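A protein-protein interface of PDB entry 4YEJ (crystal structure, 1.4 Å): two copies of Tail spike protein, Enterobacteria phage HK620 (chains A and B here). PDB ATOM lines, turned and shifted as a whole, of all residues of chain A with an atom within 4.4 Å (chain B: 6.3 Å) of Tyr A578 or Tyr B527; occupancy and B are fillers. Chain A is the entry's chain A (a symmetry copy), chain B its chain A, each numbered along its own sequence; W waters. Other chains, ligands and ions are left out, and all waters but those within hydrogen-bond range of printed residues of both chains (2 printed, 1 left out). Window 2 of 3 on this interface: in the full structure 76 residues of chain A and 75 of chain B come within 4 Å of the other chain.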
ATOM      1  N   GLN A 530      -6.451  -6.918   4.493  1.00  0.00           N
ATOM      2  CA  GLN A 530      -7.089  -5.607   4.678  1.00  0.00           C
ATOM      3  C   GLN A 530      -6.299  -4.741   5.651  1.00  0.00           C
ATOM      4  O   GLN A 530      -5.746  -5.217   6.657  1.00  0.00           O
ATOM      5  CB  GLN A 530      -8.526  -5.745   5.160  1.00  0.00           C
ATOM      6  CG  GLN A 530      -9.367  -4.481   5.097  1.00  0.00           C
ATOM      7  CD  GLN A 530      -9.187  -3.533   6.232  1.00  0.00           C
ATOM      8  OE1 GLN A 530      -8.809  -3.933   7.352  1.00  0.00           O
ATOM      9  NE2 GLN A 530      -9.386  -2.284   5.968  1.00  0.00           N
ATOM     10  N   GLY A 531      -6.244  -3.454   5.355  1.00  0.00           N
ATOM     11  CA  GLY A 531      -5.562  -2.495   6.190  1.00  0.00           C
ATOM     12  C   GLY A 531      -4.163  -2.227   5.729  1.00  0.00           C
ATOM     13  O   GLY A 531      -3.878  -2.280   4.551  1.00  0.00           O
ATOM     14  N   ALA A 532      -3.250  -1.842   6.630  1.00  0.00           N
ATOM     15  CA  ALA A 532      -1.868  -1.615   6.275  1.00  0.00           C
ATOM     16  C   ALA A 532      -1.283  -2.918   5.750  1.00  0.00           C
ATOM     17  O   ALA A 532      -1.442  -3.969   6.422  1.00  0.00           O
ATOM     18  CB  ALA A 532      -1.075  -1.128   7.489  1.00  0.00           C
ATOM     19  N   VAL A 533      -0.683  -2.885   4.570  1.00  0.00           N
ATOM     20  CA  VAL A 533      -0.360  -4.112   3.890  1.00  0.00           C
ATOM     21  C   VAL A 533       0.927  -3.881   3.102  1.00  0.00           C
ATOM     22  O   VAL A 533       1.148  -2.870   2.481  1.00  0.00           O
ATOM     23  CB  VAL A 533      -1.524  -4.533   2.955  1.00  0.00           C
ATOM     24  CG1 VAL A 533      -1.798  -3.513   1.899  1.00  0.00           C
ATOM     25  CG2 VAL A 533      -1.259  -5.897   2.378  1.00  0.00           C
ATOM     26  N   PHE A 559      -7.441   0.849  -2.710  1.00  0.00           N
ATOM     27  CA  PHE A 559      -6.138   0.664  -2.089  1.00  0.00           C
ATOM     28  C   PHE A 559      -5.206   1.731  -2.545  1.00  0.00           C
ATOM     29  O   PHE A 559      -5.456   2.419  -3.565  1.00  0.00           O
ATOM     30  CB  PHE A 559      -5.558  -0.726  -2.393  1.00  0.00           C
ATOM     31  CG  PHE A 559      -5.051  -0.920  -3.789  1.00  0.00           C
ATOM     32  CD1 PHE A 559      -5.907  -1.312  -4.810  1.00  0.00           C
ATOM     33  CD2 PHE A 559      -3.714  -0.696  -4.098  1.00  0.00           C
ATOM     34  CE1 PHE A 559      -5.385  -1.489  -6.090  1.00  0.00           C
ATOM     35  CE2 PHE A 559      -3.219  -0.916  -5.338  1.00  0.00           C
ATOM     36  CZ  PHE A 559      -4.048  -1.344  -6.336  1.00  0.00           C
ATOM     37  N   SER A 560      -4.031   1.760  -1.878  1.00  0.00           N
ATOM     38  CA  SER A 560      -2.968   2.600  -2.366  1.00  0.00           C
ATOM     39  C   SER A 560      -1.645   1.827  -2.157  1.00  0.00           C
ATOM     40  O   SER A 560      -1.452   1.234  -1.112  1.00  0.00           O
ATOM     41  CB  SER A 560      -2.936   3.964  -1.642  1.00  0.00           C
ATOM     42  OG  SER A 560      -2.909   3.761  -0.248  1.00  0.00           O
ATOM     43  N   GLY A 577       1.720  -0.132   2.180  1.00  0.00           N
ATOM     44  CA  GLY A 577       0.574   0.567   1.591  1.00  0.00           C
ATOM     45  C   GLY A 577      -0.695   0.311   2.385  1.00  0.00           C
ATOM     46  O   GLY A 577      -0.666  -0.088   3.547  1.00  0.00           O
ATOM     47  N   TYR A 578      -1.859   0.568   1.759  1.00  0.00           N
ATOM     48  CA  TYR A 578      -3.109   0.441   2.478  1.00  0.00           C
ATOM     49  C   TYR A 578      -4.213  -0.148   1.633  1.00  0.00           C
ATOM     50  O   TYR A 578      -4.554   0.439   0.633  1.00  0.00           O
ATOM     51  CB  TYR A 578      -3.579   1.813   3.103  1.00  0.00           C
ATOM     52  CG  TYR A 578      -4.695   1.626   4.089  1.00  0.00           C
ATOM     53  CD1 TYR A 578      -4.451   1.154   5.362  1.00  0.00           C
ATOM     54  CD2 TYR A 578      -6.028   1.900   3.721  1.00  0.00           C
ATOM     55  CE1 TYR A 578      -5.471   0.872   6.233  1.00  0.00           C
ATOM     56  CE2 TYR A 578      -7.029   1.680   4.602  1.00  0.00           C
ATOM     57  CZ  TYR A 578      -6.752   1.114   5.820  1.00  0.00           C
ATOM     58  OH  TYR A 578      -7.766   0.831   6.757  1.00  0.00           O
ATOM     59  N   ASN A 579      -4.761  -1.228   2.100  1.00  0.00           N
ATOM     60  CA  ASN A 579      -5.875  -1.899   1.465  1.00  0.00           C
ATOM     61  C   ASN A 579      -7.173  -1.464   2.217  1.00  0.00           C
ATOM     62  O   ASN A 579      -7.505  -2.002   3.288  1.00  0.00           O
ATOM     63  CB  ASN A 579      -5.798  -3.444   1.587  1.00  0.00           C
ATOM     64  CG  ASN A 579      -5.397  -4.160   0.272  1.00  0.00           C
ATOM     65  OD1 ASN A 579      -5.498  -3.605  -0.820  1.00  0.00           O
ATOM     66  ND2 ASN A 579      -4.917  -5.383   0.420  1.00  0.00           N
ATOM     67  N   GLU A 580      -7.976  -0.582   1.600  1.00  0.00           N
ATOM     68  CA  GLU A 580      -9.245  -0.278   2.213  1.00  0.00           C
ATOM     69  C   GLU A 580     -10.127  -1.504   2.329  1.00  0.00           C
ATOM     70  O   GLU A 580     -10.812  -1.777   3.305  1.00  0.00           O
ATOM     71  CB  GLU A 580      -9.956   0.833   1.461  1.00  0.00           C
ATOM     72  CG  GLU A 580     -11.320   1.194   1.969  1.00  0.00           C
ATOM     73  CD  GLU A 580     -11.305   1.923   3.306  1.00  0.00           C
ATOM     74  OE1 GLU A 580     -10.396   2.778   3.455  1.00  0.00           O
ATOM     75  OE2 GLU A 580     -12.245   1.597   4.128  1.00  0.00           O
ATOM     76  N   THR B 525      -7.554  13.472   8.332  1.00  0.00           N
ATOM     77  CA  THR B 525      -8.306  12.797   9.384  1.00  0.00           C
ATOM     78  C   THR B 525      -8.060  11.310   9.268  1.00  0.00           C
ATOM     79  O   THR B 525      -8.143  10.733   8.180  1.00  0.00           O
ATOM     80  CB  THR B 525      -9.780  13.143   9.287  1.00  0.00           C
ATOM     81  OG1 THR B 525      -9.912  14.533   9.677  1.00  0.00           O
ATOM     82  CG2 THR B 525     -10.653  12.289  10.252  1.00  0.00           C
ATOM     83  N   SER B 526      -7.843  10.670  10.409  1.00  0.00           N
ATOM     84  CA  SER B 526      -7.525   9.253  10.423  1.00  0.00           C
ATOM     85  C   SER B 526      -8.716   8.414  10.737  1.00  0.00           C
ATOM     86  O   SER B 526      -9.723   8.860  11.278  1.00  0.00           O
ATOM     87  CB  SER B 526      -6.446   8.938  11.469  1.00  0.00           C
ATOM     88  OG  SER B 526      -6.926   8.944  12.789  1.00  0.00           O
ATOM     89  N   TYR B 527      -8.616   7.142  10.478  1.00  0.00           N
ATOM     90  CA  TYR B 527      -9.449   6.179  11.089  1.00  0.00           C
ATOM     91  C   TYR B 527      -9.161   5.971  12.556  1.00  0.00           C
ATOM     92  O   TYR B 527      -8.183   6.508  13.107  1.00  0.00           O
ATOM     93  CB  TYR B 527      -9.406   4.808  10.345  1.00  0.00           C
ATOM     94  CG  TYR B 527      -9.965   4.786   8.946  1.00  0.00           C
ATOM     95  CD1 TYR B 527     -10.796   5.793   8.445  1.00  0.00           C
ATOM     96  CD2 TYR B 527      -9.669   3.714   8.111  1.00  0.00           C
ATOM     97  CE1 TYR B 527     -11.342   5.713   7.169  1.00  0.00           C
ATOM     98  CE2 TYR B 527     -10.167   3.662   6.824  1.00  0.00           C
ATOM     99  CZ  TYR B 527     -11.012   4.653   6.378  1.00  0.00           C
ATOM    100  OH  TYR B 527     -11.480   4.618   5.062  1.00  0.00           O
ATOM    101  N   ASN B 528     -10.047   5.265  13.255  1.00  0.00           N
ATOM    102  CA  ASN B 528      -9.884   5.150  14.731  1.00  0.00           C
ATOM    103  C   ASN B 528      -8.950   4.052  15.229  1.00  0.00           C
ATOM    104  O   ASN B 528      -8.593   4.038  16.419  1.00  0.00           O
ATOM    105  CB  ASN B 528     -11.249   5.029  15.444  1.00  0.00           C
ATOM    106  CG  ASN B 528     -11.920   3.710  15.205  1.00  0.00           C
ATOM    107  OD1 ASN B 528     -11.958   3.220  14.099  1.00  0.00           O
ATOM    108  ND2 ASN B 528     -12.522   3.169  16.239  1.00  0.00           N
ATOM    109  N   THR B 529      -8.527   3.171  14.338  1.00  0.00           N
ATOM    110  CA  THR B 529      -7.789   1.983  14.752  1.00  0.00           C
ATOM    111  C   THR B 529      -6.495   2.271  15.480  1.00  0.00           C
ATOM    112  O   THR B 529      -5.708   3.147  15.096  1.00  0.00           O
ATOM    113  CB  THR B 529      -7.406   1.185  13.507  1.00  0.00           C
ATOM    114  OG1 THR B 529      -8.416   1.405  12.463  1.00  0.00           O
ATOM    115  CG2 THR B 529      -7.337  -0.293  13.903  1.00  0.00           C
ATOM    116  N   ALA B 532      -0.949   0.836  13.182  1.00  0.00           N
ATOM    117  CA  ALA B 532      -0.789   1.447  11.882  1.00  0.00           C
ATOM    118  C   ALA B 532      -2.162   1.838  11.358  1.00  0.00           C
ATOM    119  O   ALA B 532      -3.085   0.984  11.380  1.00  0.00           O
ATOM    120  CB  ALA B 532      -0.109   0.477  10.914  1.00  0.00           C
ATOM    121  N   VAL B 533      -2.329   3.089  10.959  1.00  0.00           N
ATOM    122  CA  VAL B 533      -3.653   3.601  10.720  1.00  0.00           C
ATOM    123  C   VAL B 533      -3.560   4.617   9.584  1.00  0.00           C
ATOM    124  O   VAL B 533      -2.668   5.425   9.492  1.00  0.00           O
ATOM    125  CB  VAL B 533      -4.221   4.250  12.009  1.00  0.00           C
ATOM    126  CG1 VAL B 533      -3.392   5.401  12.477  1.00  0.00           C
ATOM    127  CG2 VAL B 533      -5.663   4.629  11.808  1.00  0.00           C
ATOM    128  N   PRO B 534      -4.545   4.570   8.635  1.00  0.00           N
ATOM    129  CA  PRO B 534      -4.479   5.522   7.550  1.00  0.00           C
ATOM    130  C   PRO B 534      -4.957   6.915   7.947  1.00  0.00           C
ATOM    131  O   PRO B 534      -5.893   7.046   8.709  1.00  0.00           O
ATOM    132  CB  PRO B 534      -5.424   4.880   6.479  1.00  0.00           C
ATOM    133  CG  PRO B 534      -6.410   4.178   7.271  1.00  0.00           C
ATOM    134  CD  PRO B 534      -5.691   3.645   8.497  1.00  0.00           C
ATOM    135  N   PHE B 535      -4.334   7.894   7.317  1.00  0.00           N
ATOM    136  CA  PHE B 535      -4.806   9.284   7.346  1.00  0.00           C
ATOM    137  C   PHE B 535      -5.185   9.695   5.920  1.00  0.00           C
ATOM    138  O   PHE B 535      -4.433   9.386   4.982  1.00  0.00           O
ATOM    139  CB  PHE B 535      -3.709  10.203   7.856  1.00  0.00           C
ATOM    140  CG  PHE B 535      -3.466  10.194   9.351  1.00  0.00           C
ATOM    141  CD1 PHE B 535      -2.929   9.086   9.998  1.00  0.00           C
ATOM    142  CD2 PHE B 535      -3.714  11.353  10.114  1.00  0.00           C
ATOM    143  CE1 PHE B 535      -2.703   9.084  11.338  1.00  0.00           C
ATOM    144  CE2 PHE B 535      -3.429  11.355  11.448  1.00  0.00           C
ATOM    145  CZ  PHE B 535      -2.951  10.236  12.060  1.00  0.00           C
ATOM    146  N   PHE B 536      -6.245  10.459   5.778  1.00  0.00           N
ATOM    147  CA  PHE B 536      -6.770  10.830   4.492  1.00  0.00           C
ATOM    148  C   PHE B 536      -7.045  12.315   4.449  1.00  0.00           C
ATOM    149  O   PHE B 536      -7.478  12.922   5.473  1.00  0.00           O
ATOM    150  CB  PHE B 536      -8.115  10.169   4.198  1.00  0.00           C
ATOM    151  CG  PHE B 536      -8.116   8.644   4.216  1.00  0.00           C
ATOM    152  CD1 PHE B 536      -7.852   7.940   3.088  1.00  0.00           C
ATOM    153  CD2 PHE B 536      -8.379   7.949   5.399  1.00  0.00           C
ATOM    154  CE1 PHE B 536      -7.856   6.548   3.088  1.00  0.00           C
ATOM    155  CE2 PHE B 536      -8.297   6.550   5.405  1.00  0.00           C
ATOM    156  CZ  PHE B 536      -8.085   5.865   4.238  1.00  0.00           C
ATOM    157  N   LYS B 568      -5.355   8.782  -4.047  1.00  0.00           N
ATOM    158  CA  LYS B 568      -6.443   7.860  -4.405  1.00  0.00           C
ATOM    159  C   LYS B 568      -7.211   8.470  -5.548  1.00  0.00           C
ATOM    160  O   LYS B 568      -7.136   9.661  -5.812  1.00  0.00           O
ATOM    161  CB  LYS B 568      -7.434   7.750  -3.213  1.00  0.00           C
ATOM    162  CG  LYS B 568      -6.928   7.058  -1.991  1.00  0.00           C
ATOM    163  CD  LYS B 568      -7.917   7.124  -0.813  1.00  0.00           C
ATOM    164  CE  LYS B 568      -9.378   6.886  -1.177  1.00  0.00           C
ATOM    165  NZ  LYS B 568     -10.236   6.807   0.073  1.00  0.00           N
ATOM    166  N   VAL B 574      -3.569   9.955   0.865  1.00  0.00           N
ATOM    167  CA  VAL B 574      -3.619   8.871   1.824  1.00  0.00           C
ATOM    168  C   VAL B 574      -2.198   8.467   2.228  1.00  0.00           C
ATOM    169  O   VAL B 574      -1.278   8.408   1.425  1.00  0.00           O
ATOM    170  CB  VAL B 574      -4.387   7.663   1.324  1.00  0.00           C
ATOM    171  CG1 VAL B 574      -3.815   7.118   0.044  1.00  0.00           C
ATOM    172  CG2 VAL B 574      -4.450   6.558   2.415  1.00  0.00           C
ATOM    173  N   GLY B 575      -2.032   8.240   3.535  1.00  0.00           N
ATOM    174  CA  GLY B 575      -0.760   7.666   4.015  1.00  0.00           C
ATOM    175  C   GLY B 575      -0.975   6.914   5.293  1.00  0.00           C
ATOM    176  O   GLY B 575      -2.035   6.974   5.879  1.00  0.00           O
ATOM    177  N   VAL B 576       0.024   6.130   5.711  1.00  0.00           N
ATOM    178  CA  VAL B 576      -0.064   5.264   6.884  1.00  0.00           C
ATOM    179  C   VAL B 576       0.719   5.834   8.041  1.00  0.00           C
ATOM    180  O   VAL B 576       1.957   6.021   7.963  1.00  0.00           O
ATOM    181  CB  VAL B 576       0.422   3.807   6.572  1.00  0.00           C
ATOM    182  CG1 VAL B 576       0.337   2.936   7.790  1.00  0.00           C
ATOM    183  CG2 VAL B 576      -0.479   3.178   5.515  1.00  0.00           C
ATOM    184  N   ASN B 579      -1.096   5.095  15.423  1.00  0.00           N
ATOM    185  CA  ASN B 579      -1.861   5.420  16.609  1.00  0.00           C
ATOM    186  C   ASN B 579      -1.303   4.546  17.778  1.00  0.00           C
ATOM    187  O   ASN B 579      -1.654   3.361  17.918  1.00  0.00           O
ATOM    188  CB  ASN B 579      -3.364   5.058  16.475  1.00  0.00           C
ATOM    189  CG  ASN B 579      -4.291   6.284  16.274  1.00  0.00           C
ATOM    190  OD1 ASN B 579      -3.925   7.421  16.565  1.00  0.00           O
ATOM    191  ND2 ASN B 579      -5.473   6.017  15.747  1.00  0.00           N
ATOM    192  N   GLY B 583      -8.093   6.174  18.315  1.00  0.00           N
ATOM    193  CA  GLY B 583      -8.905   7.355  18.210  1.00  0.00           C
ATOM    194  C   GLY B 583      -8.796   7.980  16.849  1.00  0.00           C
ATOM    195  O   GLY B 583      -7.767   7.958  16.181  1.00  0.00           O
ATOM    196  N   VAL B 584      -9.898   8.607  16.415  1.00  0.00           N
ATOM    197  CA  VAL B 584      -9.921   9.395  15.206  1.00  0.00           C
ATOM    198  C   VAL B 584      -9.074  10.646  15.417  1.00  0.00           C
ATOM    199  O   VAL B 584      -9.255  11.325  16.477  1.00  0.00           O
ATOM    200  CB  VAL B 584     -11.347   9.791  14.832  1.00  0.00           C
ATOM    201  CG1 VAL B 584     -11.387  10.812  13.721  1.00  0.00           C
ATOM    202  CG2 VAL B 584     -12.181   8.589  14.452  1.00  0.00           C
ATOM    203  N   ARG B 585      -8.143  10.884  14.528  1.00  0.00           N
ATOM    204  CA  ARG B 585      -7.261  12.055  14.639  1.00  0.00           C
ATOM    205  C   ARG B 585      -7.582  13.044  13.536  1.00  0.00           C
ATOM    206  O   ARG B 585      -8.038  12.654  12.439  1.00  0.00           O
ATOM    207  CB  ARG B 585      -5.795  11.604  14.536  1.00  0.00           C
ATOM    208  CG  ARG B 585      -5.398  10.447  15.421  1.00  0.00           C
ATOM    209  CD  ARG B 585      -5.676  10.757  16.885  1.00  0.00           C
ATOM    210  NE  ARG B 585      -5.148   9.697  17.700  1.00  0.00           N
ATOM    211  CZ  ARG B 585      -4.970   9.762  19.008  1.00  0.00           C
ATOM    212  NH1 ARG B 585      -5.337  10.860  19.661  1.00  0.00           N
ATOM    213  NH2 ARG B 585      -4.444   8.746  19.650  1.00  0.00           N
HETATM  214  O   HOH W   1      -9.755   4.266   1.173  1.00  0.00           O
HETATM  215  O   HOH W   2     -13.754   2.273   6.291  1.00  0.00           O
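The side-chain amide nitrogen (NE2) of Gln A530 sits at hydrogen-bond distance from the backbone carbonyl oxygen (O) of Glu A580, 3.1 Å away.
The backbone NH (N) of Thr B525 is in hydrogen-bond range of the backbone carbonyl oxygen (O) of Phe B536.
O of Val A533 is in hydrogen-bond range of N of Gly A577, at 2.8 Å.
O of Tyr A578 sits at hydrogen-bond distance from N of Ser A560, 2.9 Å away.
The backbone carbonyl oxygen of Pro B534 lies within hydrogen-bond range of the backbone NH of Tyr B527, 3.2 Å away.
Of the 18 printed residues of chain B, 6 touch a printed residue of chain A.
Printed residues of chain B that touch a printed residue of chain A: Tyr B527, Ala B532, Pro B534, Phe B536, Val B574 and Val B576.
Hydrophobic or aromatic side chains of chain B within 4 Å of the printed part of chain A: Tyr B527, Ala B532, Pro B534, Phe B536, Val B574 and Val B576.
Along chain B the printed residues that touch a printed residue of chain A span positions 527 to 576.
Hydrophobic or aromatic side chains of chain A that line the printed part of chain B: Ala A532 and Tyr A578.
Among the printed residues, no Asp or Glu carboxylate lies within 4 Å of a Lys or Arg side-chain nitrogen of the other chain.
The side-chain hydroxyl (OH) of Tyr B527 sits at hydrogen-bond distance from the side-chain carboxylate (OE1) of Glu A580, 2.7 Å away.
Ala A532 touches its own counterpart, Ala B532.
Positions printed for both chains: 532, 533 and 579.
Water W2 lies within hydrogen-bond range of OE2 of Glu A580 and OH of Tyr B527.
Water W1 bridges OE1 of Glu A580 (2.8 Å) and NZ of Lys B568 (2.8 Å).
Gly A531 touches none of the printed residues of chain B.
Val A533 touches none of the printed residues of chain B.
Of the printed residues of chain B, Ser A560 touches Val B574 (3.5 Å).
Of the printed residues of chain B, Tyr A578 touches Tyr B527 (3.7 Å) and Pro B534 (3.4 Å).
Of the printed residues of chain B, Glu A580 touches Tyr B527 (2.7 Å) and Phe B536 (3.9 Å).
Of the printed residues of chain A, Tyr B527 touches Tyr A578 (3.7 Å) and Glu A580 (2.7 Å).
Of the printed residues of chain A, Ala B532 touches Ala A532 (3.9 Å).
Of the printed residues of chain A, Phe B536 touches Glu A580 (3.9 Å).
Of the printed residues of chain A, Val B576 touches Gly A577.
The nearest residue of chain B that does not touch Tyr A578 is Val B576 (4.2 Å).
The nearest printed residue of chain A that does not touch Tyr B527 is Gln A530 (6.1 Å).
The nearest printed residue of chain A that does not touch Phe B536 is Tyr A578 (4.3 Å).
CB of Ala A532 touches CB of Ala B532, 3.9 Å away.
OG of Ser A560 touches CG1 of Val B574, 3.5 Å away.
Gly A577 touches Val B576.
Tyr A578 touches Tyr B527 (OH to CD2, 3.7 Å).
CZ of Tyr A578 touches CG of Pro B534, at 3.4 Å.
OE1 of Glu A580 touches CZ of Phe B536, 3.9 Å away.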
